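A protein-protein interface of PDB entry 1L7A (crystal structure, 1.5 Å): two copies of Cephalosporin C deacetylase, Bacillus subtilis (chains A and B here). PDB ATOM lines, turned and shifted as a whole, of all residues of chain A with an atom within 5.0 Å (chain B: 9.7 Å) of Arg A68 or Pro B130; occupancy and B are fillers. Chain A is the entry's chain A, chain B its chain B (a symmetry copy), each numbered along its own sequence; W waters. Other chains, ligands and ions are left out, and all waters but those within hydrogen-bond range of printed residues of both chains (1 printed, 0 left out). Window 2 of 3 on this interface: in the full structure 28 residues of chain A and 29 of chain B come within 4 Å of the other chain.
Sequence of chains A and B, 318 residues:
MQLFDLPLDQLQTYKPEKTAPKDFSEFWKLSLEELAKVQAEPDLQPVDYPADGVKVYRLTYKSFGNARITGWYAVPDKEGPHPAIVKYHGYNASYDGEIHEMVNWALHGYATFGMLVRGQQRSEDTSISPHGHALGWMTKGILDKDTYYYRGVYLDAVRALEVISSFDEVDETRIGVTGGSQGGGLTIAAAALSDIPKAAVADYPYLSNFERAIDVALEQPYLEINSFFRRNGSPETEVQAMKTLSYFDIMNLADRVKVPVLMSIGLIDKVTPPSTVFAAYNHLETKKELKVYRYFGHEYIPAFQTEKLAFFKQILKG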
ATOM      1  N   THR A  60     -12.221 -13.114 -14.531  1.00  0.00           N
ATOM      2  CA  THR A  60     -13.305 -12.866 -13.609  1.00  0.00           C
ATOM      3  C   THR A  60     -14.127 -11.709 -14.148  1.00  0.00           C
ATOM      4  O   THR A  60     -13.597 -10.724 -14.692  1.00  0.00           O
ATOM      5  CB  THR A  60     -12.805 -12.521 -12.196  1.00  0.00           C
ATOM      6  OG1 THR A  60     -12.013 -13.632 -11.765  1.00  0.00           O
ATOM      7  CG2 THR A  60     -13.942 -12.280 -11.232  1.00  0.00           C
ATOM      8  N   TYR A  61     -15.449 -11.805 -14.052  1.00  0.00           N
ATOM      9  CA  TYR A  61     -16.347 -10.750 -14.501  1.00  0.00           C
ATOM     10  C   TYR A  61     -17.573 -10.691 -13.605  1.00  0.00           C
ATOM     11  O   TYR A  61     -17.879 -11.567 -12.796  1.00  0.00           O
ATOM     12  CB  TYR A  61     -16.738 -10.903 -15.961  1.00  0.00           C
ATOM     13  CG  TYR A  61     -17.495 -12.169 -16.303  1.00  0.00           C
ATOM     14  CD1 TYR A  61     -16.843 -13.289 -16.794  1.00  0.00           C
ATOM     15  CD2 TYR A  61     -18.866 -12.211 -16.135  1.00  0.00           C
ATOM     16  CE1 TYR A  61     -17.546 -14.444 -17.109  1.00  0.00           C
ATOM     17  CE2 TYR A  61     -19.581 -13.360 -16.454  1.00  0.00           C
ATOM     18  CZ  TYR A  61     -18.910 -14.453 -16.946  1.00  0.00           C
ATOM     19  OH  TYR A  61     -19.686 -15.567 -17.235  1.00  0.00           O
ATOM     20  N   LYS A  62     -18.310  -9.596 -13.678  1.00  0.00           N
ATOM     21  CA  LYS A  62     -19.522  -9.333 -12.923  1.00  0.00           C
ATOM     22  C   LYS A  62     -20.723  -9.635 -13.812  1.00  0.00           C
ATOM     23  O   LYS A  62     -20.714  -9.359 -15.011  1.00  0.00           O
ATOM     24  CB  LYS A  62     -19.599  -7.914 -12.355  1.00  0.00           C
ATOM     25  CG  LYS A  62     -18.409  -7.535 -11.491  1.00  0.00           C
ATOM     26  CD  LYS A  62     -18.366  -8.291 -10.171  1.00  0.00           C
ATOM     27  CE  LYS A  62     -19.147  -7.507  -9.122  1.00  0.00           C
ATOM     28  NZ  LYS A  62     -19.490  -8.340  -7.938  1.00  0.00           N
ATOM     29  N   ASN A  66     -24.895  -8.905  -9.487  1.00  0.00           N
ATOM     30  CA  ASN A  66     -23.554  -8.459  -9.150  1.00  0.00           C
ATOM     31  C   ASN A  66     -22.660  -9.631  -8.765  1.00  0.00           C
ATOM     32  O   ASN A  66     -21.694  -9.451  -8.025  1.00  0.00           O
ATOM     33  CB  ASN A  66     -23.621  -7.428  -8.013  1.00  0.00           C
ATOM     34  CG  ASN A  66     -24.168  -6.118  -8.549  1.00  0.00           C
ATOM     35  OD1 ASN A  66     -23.476  -5.441  -9.303  1.00  0.00           O
ATOM     36  ND2 ASN A  66     -25.380  -5.732  -8.198  1.00  0.00           N
ATOM     37  N   ALA A  67     -22.978 -10.812  -9.307  1.00  0.00           N
ATOM     38  CA  ALA A  67     -22.172 -11.985  -8.957  1.00  0.00           C
ATOM     39  C   ALA A  67     -20.836 -12.002  -9.665  1.00  0.00           C
ATOM     40  O   ALA A  67     -20.707 -11.679 -10.839  1.00  0.00           O
ATOM     41  CB  ALA A  67     -22.950 -13.261  -9.287  1.00  0.00           C
ATOM     42  N   ARG A  68     -19.805 -12.414  -8.939  1.00  0.00           N
ATOM     43  CA  ARG A  68     -18.455 -12.568  -9.446  1.00  0.00           C
ATOM     44  C   ARG A  68     -18.329 -13.974 -10.038  1.00  0.00           C
ATOM     45  O   ARG A  68     -18.287 -14.991  -9.342  1.00  0.00           O
ATOM     46  CB  ARG A  68     -17.487 -12.397  -8.288  1.00  0.00           C
ATOM     47  CG  ARG A  68     -16.014 -12.597  -8.568  1.00  0.00           C
ATOM     48  CD  ARG A  68     -15.234 -12.627  -7.254  1.00  0.00           C
ATOM     49  NE  ARG A  68     -15.283 -13.936  -6.606  1.00  0.00           N
ATOM     50  CZ  ARG A  68     -14.422 -14.343  -5.679  1.00  0.00           C
ATOM     51  NH1 ARG A  68     -13.431 -13.559  -5.266  1.00  0.00           N
ATOM     52  NH2 ARG A  68     -14.531 -15.555  -5.137  1.00  0.00           N
ATOM     53  N   ILE A  69     -18.240 -14.032 -11.358  1.00  0.00           N
ATOM     54  CA  ILE A  69     -18.136 -15.265 -12.113  1.00  0.00           C
ATOM     55  C   ILE A  69     -16.702 -15.401 -12.590  1.00  0.00           C
ATOM     56  O   ILE A  69     -16.106 -14.408 -13.044  1.00  0.00           O
ATOM     57  CB  ILE A  69     -19.098 -15.223 -13.305  1.00  0.00           C
ATOM     58  CG1 ILE A  69     -20.499 -14.862 -12.830  1.00  0.00           C
ATOM     59  CG2 ILE A  69     -19.133 -16.563 -14.030  1.00  0.00           C
ATOM     60  CD1 ILE A  69     -21.087 -15.777 -11.775  1.00  0.00           C
ATOM     61  N   THR A  70     -16.154 -16.599 -12.546  1.00  0.00           N
ATOM     62  CA  THR A  70     -14.773 -16.807 -12.935  1.00  0.00           C
ATOM     63  C   THR A  70     -14.558 -18.126 -13.647  1.00  0.00           C
ATOM     64  O   THR A  70     -15.485 -18.938 -13.762  1.00  0.00           O
ATOM     65  CB  THR A  70     -13.941 -16.702 -11.637  1.00  0.00           C
ATOM     66  OG1 THR A  70     -12.552 -16.528 -11.956  1.00  0.00           O
ATOM     67  CG2 THR A  70     -14.080 -17.934 -10.754  1.00  0.00           C
ATOM     68  N   ARG A 122     -15.914 -22.049  -7.408  1.00  0.00           N
ATOM     69  CA  ARG A 122     -15.220 -20.773  -7.567  1.00  0.00           C
ATOM     70  C   ARG A 122     -16.192 -19.602  -7.756  1.00  0.00           C
ATOM     71  O   ARG A 122     -16.073 -18.566  -7.119  1.00  0.00           O
ATOM     72  CB  ARG A 122     -14.278 -20.875  -8.770  1.00  0.00           C
ATOM     73  CG  ARG A 122     -12.974 -21.600  -8.428  1.00  0.00           C
ATOM     74  CD  ARG A 122     -11.964 -21.541  -9.581  1.00  0.00           C
ATOM     75  NE  ARG A 122     -11.468 -22.886  -9.901  1.00  0.00           N
ATOM     76  CZ  ARG A 122     -10.196 -23.179  -9.569  1.00  0.00           C
ATOM     77  NH1 ARG A 122      -9.227 -22.314  -9.809  1.00  0.00           N
ATOM     78  NH2 ARG A 122      -9.928 -24.340  -8.963  1.00  0.00           N
ATOM     79  N   SER A 123     -17.091 -19.584  -8.718  1.00  0.00           N
ATOM     80  CA  SER A 123     -17.975 -18.468  -8.986  1.00  0.00           C
ATOM     81  C   SER A 123     -19.001 -18.325  -7.871  1.00  0.00           C
ATOM     82  O   SER A 123     -19.486 -19.290  -7.271  1.00  0.00           O
ATOM     83  CB  SER A 123     -18.679 -18.672 -10.321  1.00  0.00           C
ATOM     84  OG  SER A 123     -17.707 -18.695 -11.344  1.00  0.00           O
ATOM     85  N   GLU A 124     -19.305 -17.070  -7.558  1.00  0.00           N
ATOM     86  CA  GLU A 124     -20.253 -16.727  -6.520  1.00  0.00           C
ATOM     87  C   GLU A 124     -21.709 -16.746  -6.969  1.00  0.00           C
ATOM     88  O   GLU A 124     -22.018 -16.348  -8.090  1.00  0.00           O
ATOM     89  CB  GLU A 124     -19.873 -15.306  -6.100  1.00  0.00           C
ATOM     90  CG  GLU A 124     -20.821 -14.548  -5.199  1.00  0.00           C
ATOM     91  CD  GLU A 124     -20.253 -13.139  -5.074  1.00  0.00           C
ATOM     92  OE1 GLU A 124     -20.145 -12.377  -6.057  1.00  0.00           O
ATOM     93  OE2 GLU A 124     -19.905 -12.817  -3.918  1.00  0.00           O
ATOM     94  N   ASP B 125     -32.703 -18.707   3.331  1.00  0.00           N
ATOM     95  CA  ASP B 125     -31.283 -18.575   3.638  1.00  0.00           C
ATOM     96  C   ASP B 125     -30.838 -17.365   2.818  1.00  0.00           C
ATOM     97  O   ASP B 125     -30.700 -17.450   1.597  1.00  0.00           O
ATOM     98  CB  ASP B 125     -30.435 -19.786   3.290  1.00  0.00           C
ATOM     99  CG  ASP B 125     -28.963 -19.577   3.609  1.00  0.00           C
ATOM    100  OD1 ASP B 125     -28.174 -20.462   3.220  1.00  0.00           O
ATOM    101  OD2 ASP B 125     -28.585 -18.556   4.222  1.00  0.00           O
ATOM    102  N   THR B 126     -30.694 -16.206   3.469  1.00  0.00           N
ATOM    103  CA  THR B 126     -30.249 -14.995   2.791  1.00  0.00           C
ATOM    104  C   THR B 126     -28.738 -14.938   2.641  1.00  0.00           C
ATOM    105  O   THR B 126     -28.255 -13.990   2.011  1.00  0.00           O
ATOM    106  CB  THR B 126     -30.713 -13.703   3.487  1.00  0.00           C
ATOM    107  OG1 THR B 126     -30.214 -13.735   4.834  1.00  0.00           O
ATOM    108  CG2 THR B 126     -32.220 -13.618   3.559  1.00  0.00           C
ATOM    109  N   SER B 127     -27.984 -15.879   3.210  1.00  0.00           N
ATOM    110  CA  SER B 127     -26.531 -15.869   3.032  1.00  0.00           C
ATOM    111  C   SER B 127     -26.191 -16.342   1.618  1.00  0.00           C
ATOM    112  O   SER B 127     -26.805 -17.296   1.134  1.00  0.00           O
ATOM    113  CB  SER B 127     -25.826 -16.644   4.130  1.00  0.00           C
ATOM    114  OG  SER B 127     -25.955 -18.037   3.948  1.00  0.00           O
ATOM    115  N   ILE B 128     -25.265 -15.679   0.941  1.00  0.00           N
ATOM    116  CA  ILE B 128     -24.936 -16.047  -0.432  1.00  0.00           C
ATOM    117  C   ILE B 128     -24.024 -17.268  -0.476  1.00  0.00           C
ATOM    118  O   ILE B 128     -23.706 -17.841   0.557  1.00  0.00           O
ATOM    119  CB  ILE B 128     -24.240 -14.860  -1.133  1.00  0.00           C
ATOM    120  CG1 ILE B 128     -22.899 -14.520  -0.503  1.00  0.00           C
ATOM    121  CG2 ILE B 128     -25.201 -13.677  -1.100  1.00  0.00           C
ATOM    122  CD1 ILE B 128     -21.939 -13.781  -1.411  1.00  0.00           C
ATOM    123  N   SER B 129     -23.598 -17.651  -1.667  1.00  0.00           N
ATOM    124  CA  SER B 129     -22.625 -18.726  -1.869  1.00  0.00           C
ATOM    125  C   SER B 129     -21.399 -17.969  -2.393  1.00  0.00           C
ATOM    126  O   SER B 129     -21.264 -17.714  -3.592  1.00  0.00           O
ATOM    127  CB  SER B 129     -23.106 -19.733  -2.902  1.00  0.00           C
ATOM    128  OG  SER B 129     -24.385 -20.230  -2.541  1.00  0.00           O
ATOM    129  N   PRO B 130     -20.480 -17.604  -1.492  1.00  0.00           N
ATOM    130  CA  PRO B 130     -19.323 -16.817  -1.874  1.00  0.00           C
ATOM    131  C   PRO B 130     -18.215 -17.364  -2.748  1.00  0.00           C
ATOM    132  O   PRO B 130     -17.584 -16.602  -3.485  1.00  0.00           O
ATOM    133  CB  PRO B 130     -18.772 -16.412  -0.504  1.00  0.00           C
ATOM    134  CG  PRO B 130     -19.224 -17.451   0.456  1.00  0.00           C
ATOM    135  CD  PRO B 130     -20.585 -17.875  -0.041  1.00  0.00           C
ATOM    136  N   HIS B 131     -18.031 -18.681  -2.735  1.00  0.00           N
ATOM    137  CA  HIS B 131     -16.959 -19.293  -3.506  1.00  0.00           C
ATOM    138  C   HIS B 131     -17.232 -20.625  -4.197  1.00  0.00           C
ATOM    139  O   HIS B 131     -16.272 -21.156  -4.764  1.00  0.00           O
ATOM    140  CB  HIS B 131     -15.815 -19.519  -2.510  1.00  0.00           C
ATOM    141  CG  HIS B 131     -16.168 -20.260  -1.260  1.00  0.00           C
ATOM    142  ND1 HIS B 131     -16.593 -21.572  -1.241  1.00  0.00           N
ATOM    143  CD2 HIS B 131     -16.129 -19.858   0.028  1.00  0.00           C
ATOM    144  CE1 HIS B 131     -16.820 -21.934   0.015  1.00  0.00           C
ATOM    145  NE2 HIS B 131     -16.539 -20.914   0.812  1.00  0.00           N
ATOM    146  N   GLY B 132     -18.486 -21.070  -4.203  1.00  0.00           N
ATOM    147  CA  GLY B 132     -18.760 -22.348  -4.872  1.00  0.00           C
ATOM    148  C   GLY B 132     -18.518 -23.469  -3.869  1.00  0.00           C
ATOM    149  O   GLY B 132     -17.559 -23.415  -3.091  1.00  0.00           O
ATOM    150  N   HIS B 133     -19.377 -24.480  -3.883  1.00  0.00           N
ATOM    151  CA  HIS B 133     -19.246 -25.574  -2.927  1.00  0.00           C
ATOM    152  C   HIS B 133     -19.710 -26.895  -3.538  1.00  0.00           C
ATOM    153  O   HIS B 133     -20.322 -26.889  -4.605  1.00  0.00           O
ATOM    154  CB  HIS B 133     -20.096 -25.271  -1.684  1.00  0.00           C
ATOM    155  CG  HIS B 133     -21.540 -24.967  -1.952  1.00  0.00           C
ATOM    156  ND1 HIS B 133     -22.461 -25.979  -2.094  1.00  0.00           N
ATOM    157  CD2 HIS B 133     -22.243 -23.814  -2.115  1.00  0.00           C
ATOM    158  CE1 HIS B 133     -23.660 -25.475  -2.308  1.00  0.00           C
ATOM    159  NE2 HIS B 133     -23.554 -24.163  -2.349  1.00  0.00           N
ATOM    160  N   TRP B 137     -25.234 -28.410   1.525  1.00  0.00           N
ATOM    161  CA  TRP B 137     -25.009 -27.214   2.322  1.00  0.00           C
ATOM    162  C   TRP B 137     -23.763 -27.288   3.205  1.00  0.00           C
ATOM    163  O   TRP B 137     -23.347 -26.243   3.709  1.00  0.00           O
ATOM    164  CB  TRP B 137     -26.215 -26.951   3.237  1.00  0.00           C
ATOM    165  CG  TRP B 137     -27.524 -26.649   2.565  1.00  0.00           C
ATOM    166  CD1 TRP B 137     -27.988 -25.423   2.162  1.00  0.00           C
ATOM    167  CD2 TRP B 137     -28.560 -27.586   2.240  1.00  0.00           C
ATOM    168  NE1 TRP B 137     -29.247 -25.548   1.621  1.00  0.00           N
ATOM    169  CE2 TRP B 137     -29.608 -26.865   1.636  1.00  0.00           C
ATOM    170  CE3 TRP B 137     -28.681 -28.970   2.367  1.00  0.00           C
ATOM    171  CZ2 TRP B 137     -30.775 -27.487   1.182  1.00  0.00           C
ATOM    172  CZ3 TRP B 137     -29.861 -29.569   1.955  1.00  0.00           C
ATOM    173  CH2 TRP B 137     -30.881 -28.838   1.328  1.00  0.00           C
ATOM    174  N   THR B 139     -20.600 -27.435   2.698  1.00  0.00           N
ATOM    175  CA  THR B 139     -19.421 -26.651   2.341  1.00  0.00           C
ATOM    176  C   THR B 139     -19.739 -25.249   1.868  1.00  0.00           C
ATOM    177  O   THR B 139     -18.849 -24.550   1.363  1.00  0.00           O
ATOM    178  CB  THR B 139     -18.529 -27.461   1.367  1.00  0.00           C
ATOM    179  OG1 THR B 139     -19.206 -27.837   0.159  1.00  0.00           O
ATOM    180  CG2 THR B 139     -18.066 -28.717   2.097  1.00  0.00           C
ATOM    181  N   LYS B 140     -21.011 -24.850   1.913  1.00  0.00           N
ATOM    182  CA  LYS B 140     -21.426 -23.516   1.499  1.00  0.00           C
ATOM    183  C   LYS B 140     -20.791 -22.468   2.424  1.00  0.00           C
ATOM    184  O   LYS B 140     -21.060 -22.458   3.636  1.00  0.00           O
ATOM    185  CB  LYS B 140     -22.961 -23.444   1.490  1.00  0.00           C
ATOM    186  CG  LYS B 140     -23.517 -22.072   1.141  1.00  0.00           C
ATOM    187  CD  LYS B 140     -25.028 -22.185   0.923  1.00  0.00           C
ATOM    188  CE  LYS B 140     -25.638 -20.852   0.530  1.00  0.00           C
ATOM    189  NZ  LYS B 140     -25.689 -19.931   1.714  1.00  0.00           N
ATOM    190  N   GLY B 141     -19.940 -21.632   1.821  1.00  0.00           N
ATOM    191  CA  GLY B 141     -19.259 -20.601   2.607  1.00  0.00           C
ATOM    192  C   GLY B 141     -18.198 -21.101   3.567  1.00  0.00           C
ATOM    193  O   GLY B 141     -17.783 -20.359   4.469  1.00  0.00           O
ATOM    194  N   ILE B 142     -17.750 -22.337   3.420  1.00  0.00           N
ATOM    195  CA  ILE B 142     -16.773 -22.946   4.314  1.00  0.00           C
ATOM    196  C   ILE B 142     -15.399 -22.280   4.347  1.00  0.00           C
ATOM    197  O   ILE B 142     -14.679 -22.612   5.313  1.00  0.00           O
ATOM    198  CB  ILE B 142     -16.689 -24.453   3.966  1.00  0.00           C
ATOM    199  CG1 ILE B 142     -16.166 -25.244   5.170  1.00  0.00           C
ATOM    200  CG2 ILE B 142     -15.843 -24.723   2.741  1.00  0.00           C
ATOM    201  CD1 ILE B 142     -16.239 -26.755   5.043  1.00  0.00           C
ATOM    202  N   LEU B 143     -15.093 -21.415   3.381  1.00  0.00           N
ATOM    203  CA  LEU B 143     -13.755 -20.803   3.460  1.00  0.00           C
ATOM    204  C   LEU B 143     -13.677 -19.654   4.444  1.00  0.00           C
ATOM    205  O   LEU B 143     -12.584 -19.091   4.581  1.00  0.00           O
ATOM    206  CB  LEU B 143     -13.274 -20.422   2.064  1.00  0.00           C
ATOM    207  CG  LEU B 143     -13.211 -21.640   1.131  1.00  0.00           C
ATOM    208  CD1 LEU B 143     -12.721 -21.187  -0.232  1.00  0.00           C
ATOM    209  CD2 LEU B 143     -12.323 -22.727   1.715  1.00  0.00           C
ATOM    210  N   ASP B 144     -14.745 -19.285   5.129  1.00  0.00           N
ATOM    211  CA  ASP B 144     -14.687 -18.217   6.116  1.00  0.00           C
ATOM    212  C   ASP B 144     -15.777 -18.410   7.162  1.00  0.00           C
ATOM    213  O   ASP B 144     -16.937 -18.551   6.776  1.00  0.00           O
ATOM    214  CB  ASP B 144     -14.828 -16.855   5.439  1.00  0.00           C
ATOM    215  CG  ASP B 144     -14.709 -15.596   6.260  1.00  0.00           C
ATOM    216  OD1 ASP B 144     -14.887 -15.515   7.486  1.00  0.00           O
ATOM    217  OD2 ASP B 144     -14.421 -14.558   5.614  1.00  0.00           O
ATOM    218  N   LYS B 145     -15.427 -18.409   8.439  1.00  0.00           N
ATOM    219  CA  LYS B 145     -16.422 -18.558   9.490  1.00  0.00           C
ATOM    220  C   LYS B 145     -17.593 -17.582   9.357  1.00  0.00           C
ATOM    221  O   LYS B 145     -18.733 -17.920   9.718  1.00  0.00           O
ATOM    222  CB  LYS B 145     -15.747 -18.369  10.850  1.00  0.00           C
ATOM    223  CG  LYS B 145     -15.133 -16.982  11.035  1.00  0.00           C
ATOM    224  CD  LYS B 145     -14.278 -17.034  12.293  1.00  0.00           C
ATOM    225  CE  LYS B 145     -13.706 -15.706  12.746  1.00  0.00           C
ATOM    226  NZ  LYS B 145     -12.688 -15.198  11.796  1.00  0.00           N
ATOM    227  N   ASP B 146     -17.328 -16.378   8.846  1.00  0.00           N
ATOM    228  CA  ASP B 146     -18.391 -15.390   8.720  1.00  0.00           C
ATOM    229  C   ASP B 146     -19.436 -15.714   7.657  1.00  0.00           C
ATOM    230  O   ASP B 146     -20.593 -15.318   7.806  1.00  0.00           O
ATOM    231  CB  ASP B 146     -17.791 -14.006   8.436  1.00  0.00           C
ATOM    232  CG  ASP B 146     -17.136 -13.360   9.639  1.00  0.00           C
ATOM    233  OD1 ASP B 146     -17.372 -13.787  10.777  1.00  0.00           O
ATOM    234  OD2 ASP B 146     -16.371 -12.393   9.398  1.00  0.00           O
ATOM    235  N   THR B 147     -19.031 -16.466   6.640  1.00  0.00           N
ATOM    236  CA  THR B 147     -19.919 -16.820   5.545  1.00  0.00           C
ATOM    237  C   THR B 147     -20.392 -18.269   5.598  1.00  0.00           C
ATOM    238  O   THR B 147     -21.298 -18.617   4.831  1.00  0.00           O
ATOM    239  CB  THR B 147     -19.166 -16.692   4.196  1.00  0.00           C
ATOM    240  OG1 THR B 147     -17.974 -17.493   4.136  1.00  0.00           O
ATOM    241  CG2 THR B 147     -18.705 -15.270   3.905  1.00  0.00           C
ATOM    242  N   TYR B 148     -19.936 -19.006   6.598  1.00  0.00           N
ATOM    243  CA  TYR B 148     -20.288 -20.430   6.647  1.00  0.00           C
ATOM    244  C   TYR B 148     -21.770 -20.657   6.891  1.00  0.00           C
ATOM    245  O   TYR B 148     -22.384 -20.022   7.748  1.00  0.00           O
ATOM    246  CB  TYR B 148     -19.404 -21.166   7.662  1.00  0.00           C
ATOM    247  CG  TYR B 148     -19.665 -22.662   7.596  1.00  0.00           C
ATOM    248  CD1 TYR B 148     -19.556 -23.359   6.405  1.00  0.00           C
ATOM    249  CD2 TYR B 148     -20.034 -23.351   8.744  1.00  0.00           C
ATOM    250  CE1 TYR B 148     -19.827 -24.716   6.341  1.00  0.00           C
ATOM    251  CE2 TYR B 148     -20.270 -24.722   8.696  1.00  0.00           C
ATOM    252  CZ  TYR B 148     -20.183 -25.385   7.489  1.00  0.00           C
ATOM    253  OH  TYR B 148     -20.450 -26.738   7.500  1.00  0.00           O
ATOM    254  N   TYR B 149     -22.329 -21.637   6.166  1.00  0.00           N
ATOM    255  CA  TYR B 149     -23.743 -21.958   6.299  1.00  0.00           C
ATOM    256  C   TYR B 149     -24.271 -22.103   7.709  1.00  0.00           C
ATOM    257  O   TYR B 149     -25.326 -21.517   7.996  1.00  0.00           O
ATOM    258  CB  TYR B 149     -23.975 -23.284   5.556  1.00  0.00           C
ATOM    259  CG  TYR B 149     -25.403 -23.771   5.609  1.00  0.00           C
ATOM    260  CD1 TYR B 149     -26.427 -23.073   4.985  1.00  0.00           C
ATOM    261  CD2 TYR B 149     -25.713 -24.949   6.269  1.00  0.00           C
ATOM    262  CE1 TYR B 149     -27.735 -23.539   5.020  1.00  0.00           C
ATOM    263  CE2 TYR B 149     -27.023 -25.424   6.321  1.00  0.00           C
ATOM    264  CZ  TYR B 149     -28.003 -24.709   5.682  1.00  0.00           C
ATOM    265  OH  TYR B 149     -29.290 -25.195   5.724  1.00  0.00           O
ATOM    266  N   PHE B 228     -15.872 -31.705  -1.445  1.00  0.00           N
ATOM    267  CA  PHE B 228     -15.400 -30.339  -1.663  1.00  0.00           C
ATOM    268  C   PHE B 228     -13.895 -30.344  -1.838  1.00  0.00           C
ATOM    269  O   PHE B 228     -13.388 -29.657  -2.740  1.00  0.00           O
ATOM    270  CB  PHE B 228     -15.860 -29.438  -0.507  1.00  0.00           C
ATOM    271  CG  PHE B 228     -15.320 -28.032  -0.533  1.00  0.00           C
ATOM    272  CD1 PHE B 228     -15.876 -27.109  -1.404  1.00  0.00           C
ATOM    273  CD2 PHE B 228     -14.286 -27.639   0.301  1.00  0.00           C
ATOM    274  CE1 PHE B 228     -15.403 -25.803  -1.438  1.00  0.00           C
ATOM    275  CE2 PHE B 228     -13.811 -26.348   0.254  1.00  0.00           C
ATOM    276  CZ  PHE B 228     -14.360 -25.418  -0.606  1.00  0.00           C
ATOM    277  N   ASN B 232     -11.778 -28.875  -4.949  1.00  0.00           N
ATOM    278  CA  ASN B 232     -11.009 -27.671  -4.654  1.00  0.00           C
ATOM    279  C   ASN B 232      -9.818 -28.234  -3.902  1.00  0.00           C
ATOM    280  O   ASN B 232      -9.778 -28.280  -2.667  1.00  0.00           O
ATOM    281  CB  ASN B 232     -11.870 -26.788  -3.756  1.00  0.00           C
ATOM    282  CG  ASN B 232     -13.221 -26.435  -4.335  1.00  0.00           C
ATOM    283  OD1 ASN B 232     -14.198 -27.197  -4.218  1.00  0.00           O
ATOM    284  ND2 ASN B 232     -13.255 -25.294  -4.983  1.00  0.00           N
HETATM  285  O   HOH W   1     -15.562 -23.845  -5.411  1.00  0.00           O
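The side-chain carboxylate (OE1) of Glu A124 sits at hydrogen-bond distance from the backbone NH (N) of Arg A68, 2.9 Å away.
N of Thr A70 is in hydrogen-bond range of OG of Ser A123.
The backbone carbonyl oxygen (O) of Ile B128 sits at hydrogen-bond distance from the side-chain amino group (NZ) of Lys B140 (3.1 Å).
The backbone NH (N) of Ile B142 sits at hydrogen-bond distance from a ring nitrogen (NE2) of His B131 (3.2 Å).
A ring nitrogen (NE2) of His B131 is in hydrogen-bond range of the backbone NH of Leu B143 (3.0 Å).
The backbone carbonyl oxygen of His B131 lies within hydrogen-bond range of the backbone NH of Arg A122 (2.8 Å).
No residue of chain B comes within 4 Å of Ala A67.
Arg A68 touches just one residue of chain B: Pro B130.
No residue of chain B comes within 4 Å of Ile A69.
Of the printed residues of chain B, Arg A122 touches His B131 (2.8 Å) and Gly B132 (3.8 Å).
Of chain B, only Gly B132 comes within 4 Å of Ser A123.
Glu A124 touches just these residues of chain B: Ile B128, Ser B129 and Pro B130.
Printed residues of chain A within 4 Å of Ile B128: Glu A124.
Printed residues of chain A within 4 Å of Ser B129: Glu A124.
Of chain A, only Arg A68 (3.6 Å) and Glu A124 (3.7 Å) come within 4 Å of Pro B130.
Of the printed residues of chain A, His B131 touches Arg A122.
The nearest residue of chain B that does not touch Arg A68 is His B131 (4.7 Å).
The nearest printed residue of chain A that does not touch Ile B128 is Ala A67 (7.8 Å).
Of the 11 printed residues of chain A, 4 touch a printed residue of chain B.
Hydrophobic or aromatic side chains of chain B that line the printed part of chain A: Ile B128.
Among the printed residues, 7 pairs touch across the chains.
Among the printed residues, no Asp or Glu carboxylate lies within 4 Å of a Lys or Arg side-chain nitrogen of the other chain.
No position is printed for both chains.
Of the 7 pairs that touch across the chains among the printed residues, none has its exchanged pair printed and touching as well.
Among the printed residues, merely in contact across the chains: Arg A68 with Pro B130, Arg A122 with Gly B132, Ser A123 with Gly B132, Glu A124 with Ile B128, Glu A124 with Ser B129 and Glu A124 with Pro B130.
Water W1 lies within hydrogen-bond range of the backbone NH of Arg A122 (2.7 Å), the side-chain amide nitrogen of Asn B232 (2.8 Å), the backbone carbonyl oxygen of His B131 (2.9 Å) and the backbone carbonyl oxygen of Gly B132 (3.1 Å).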
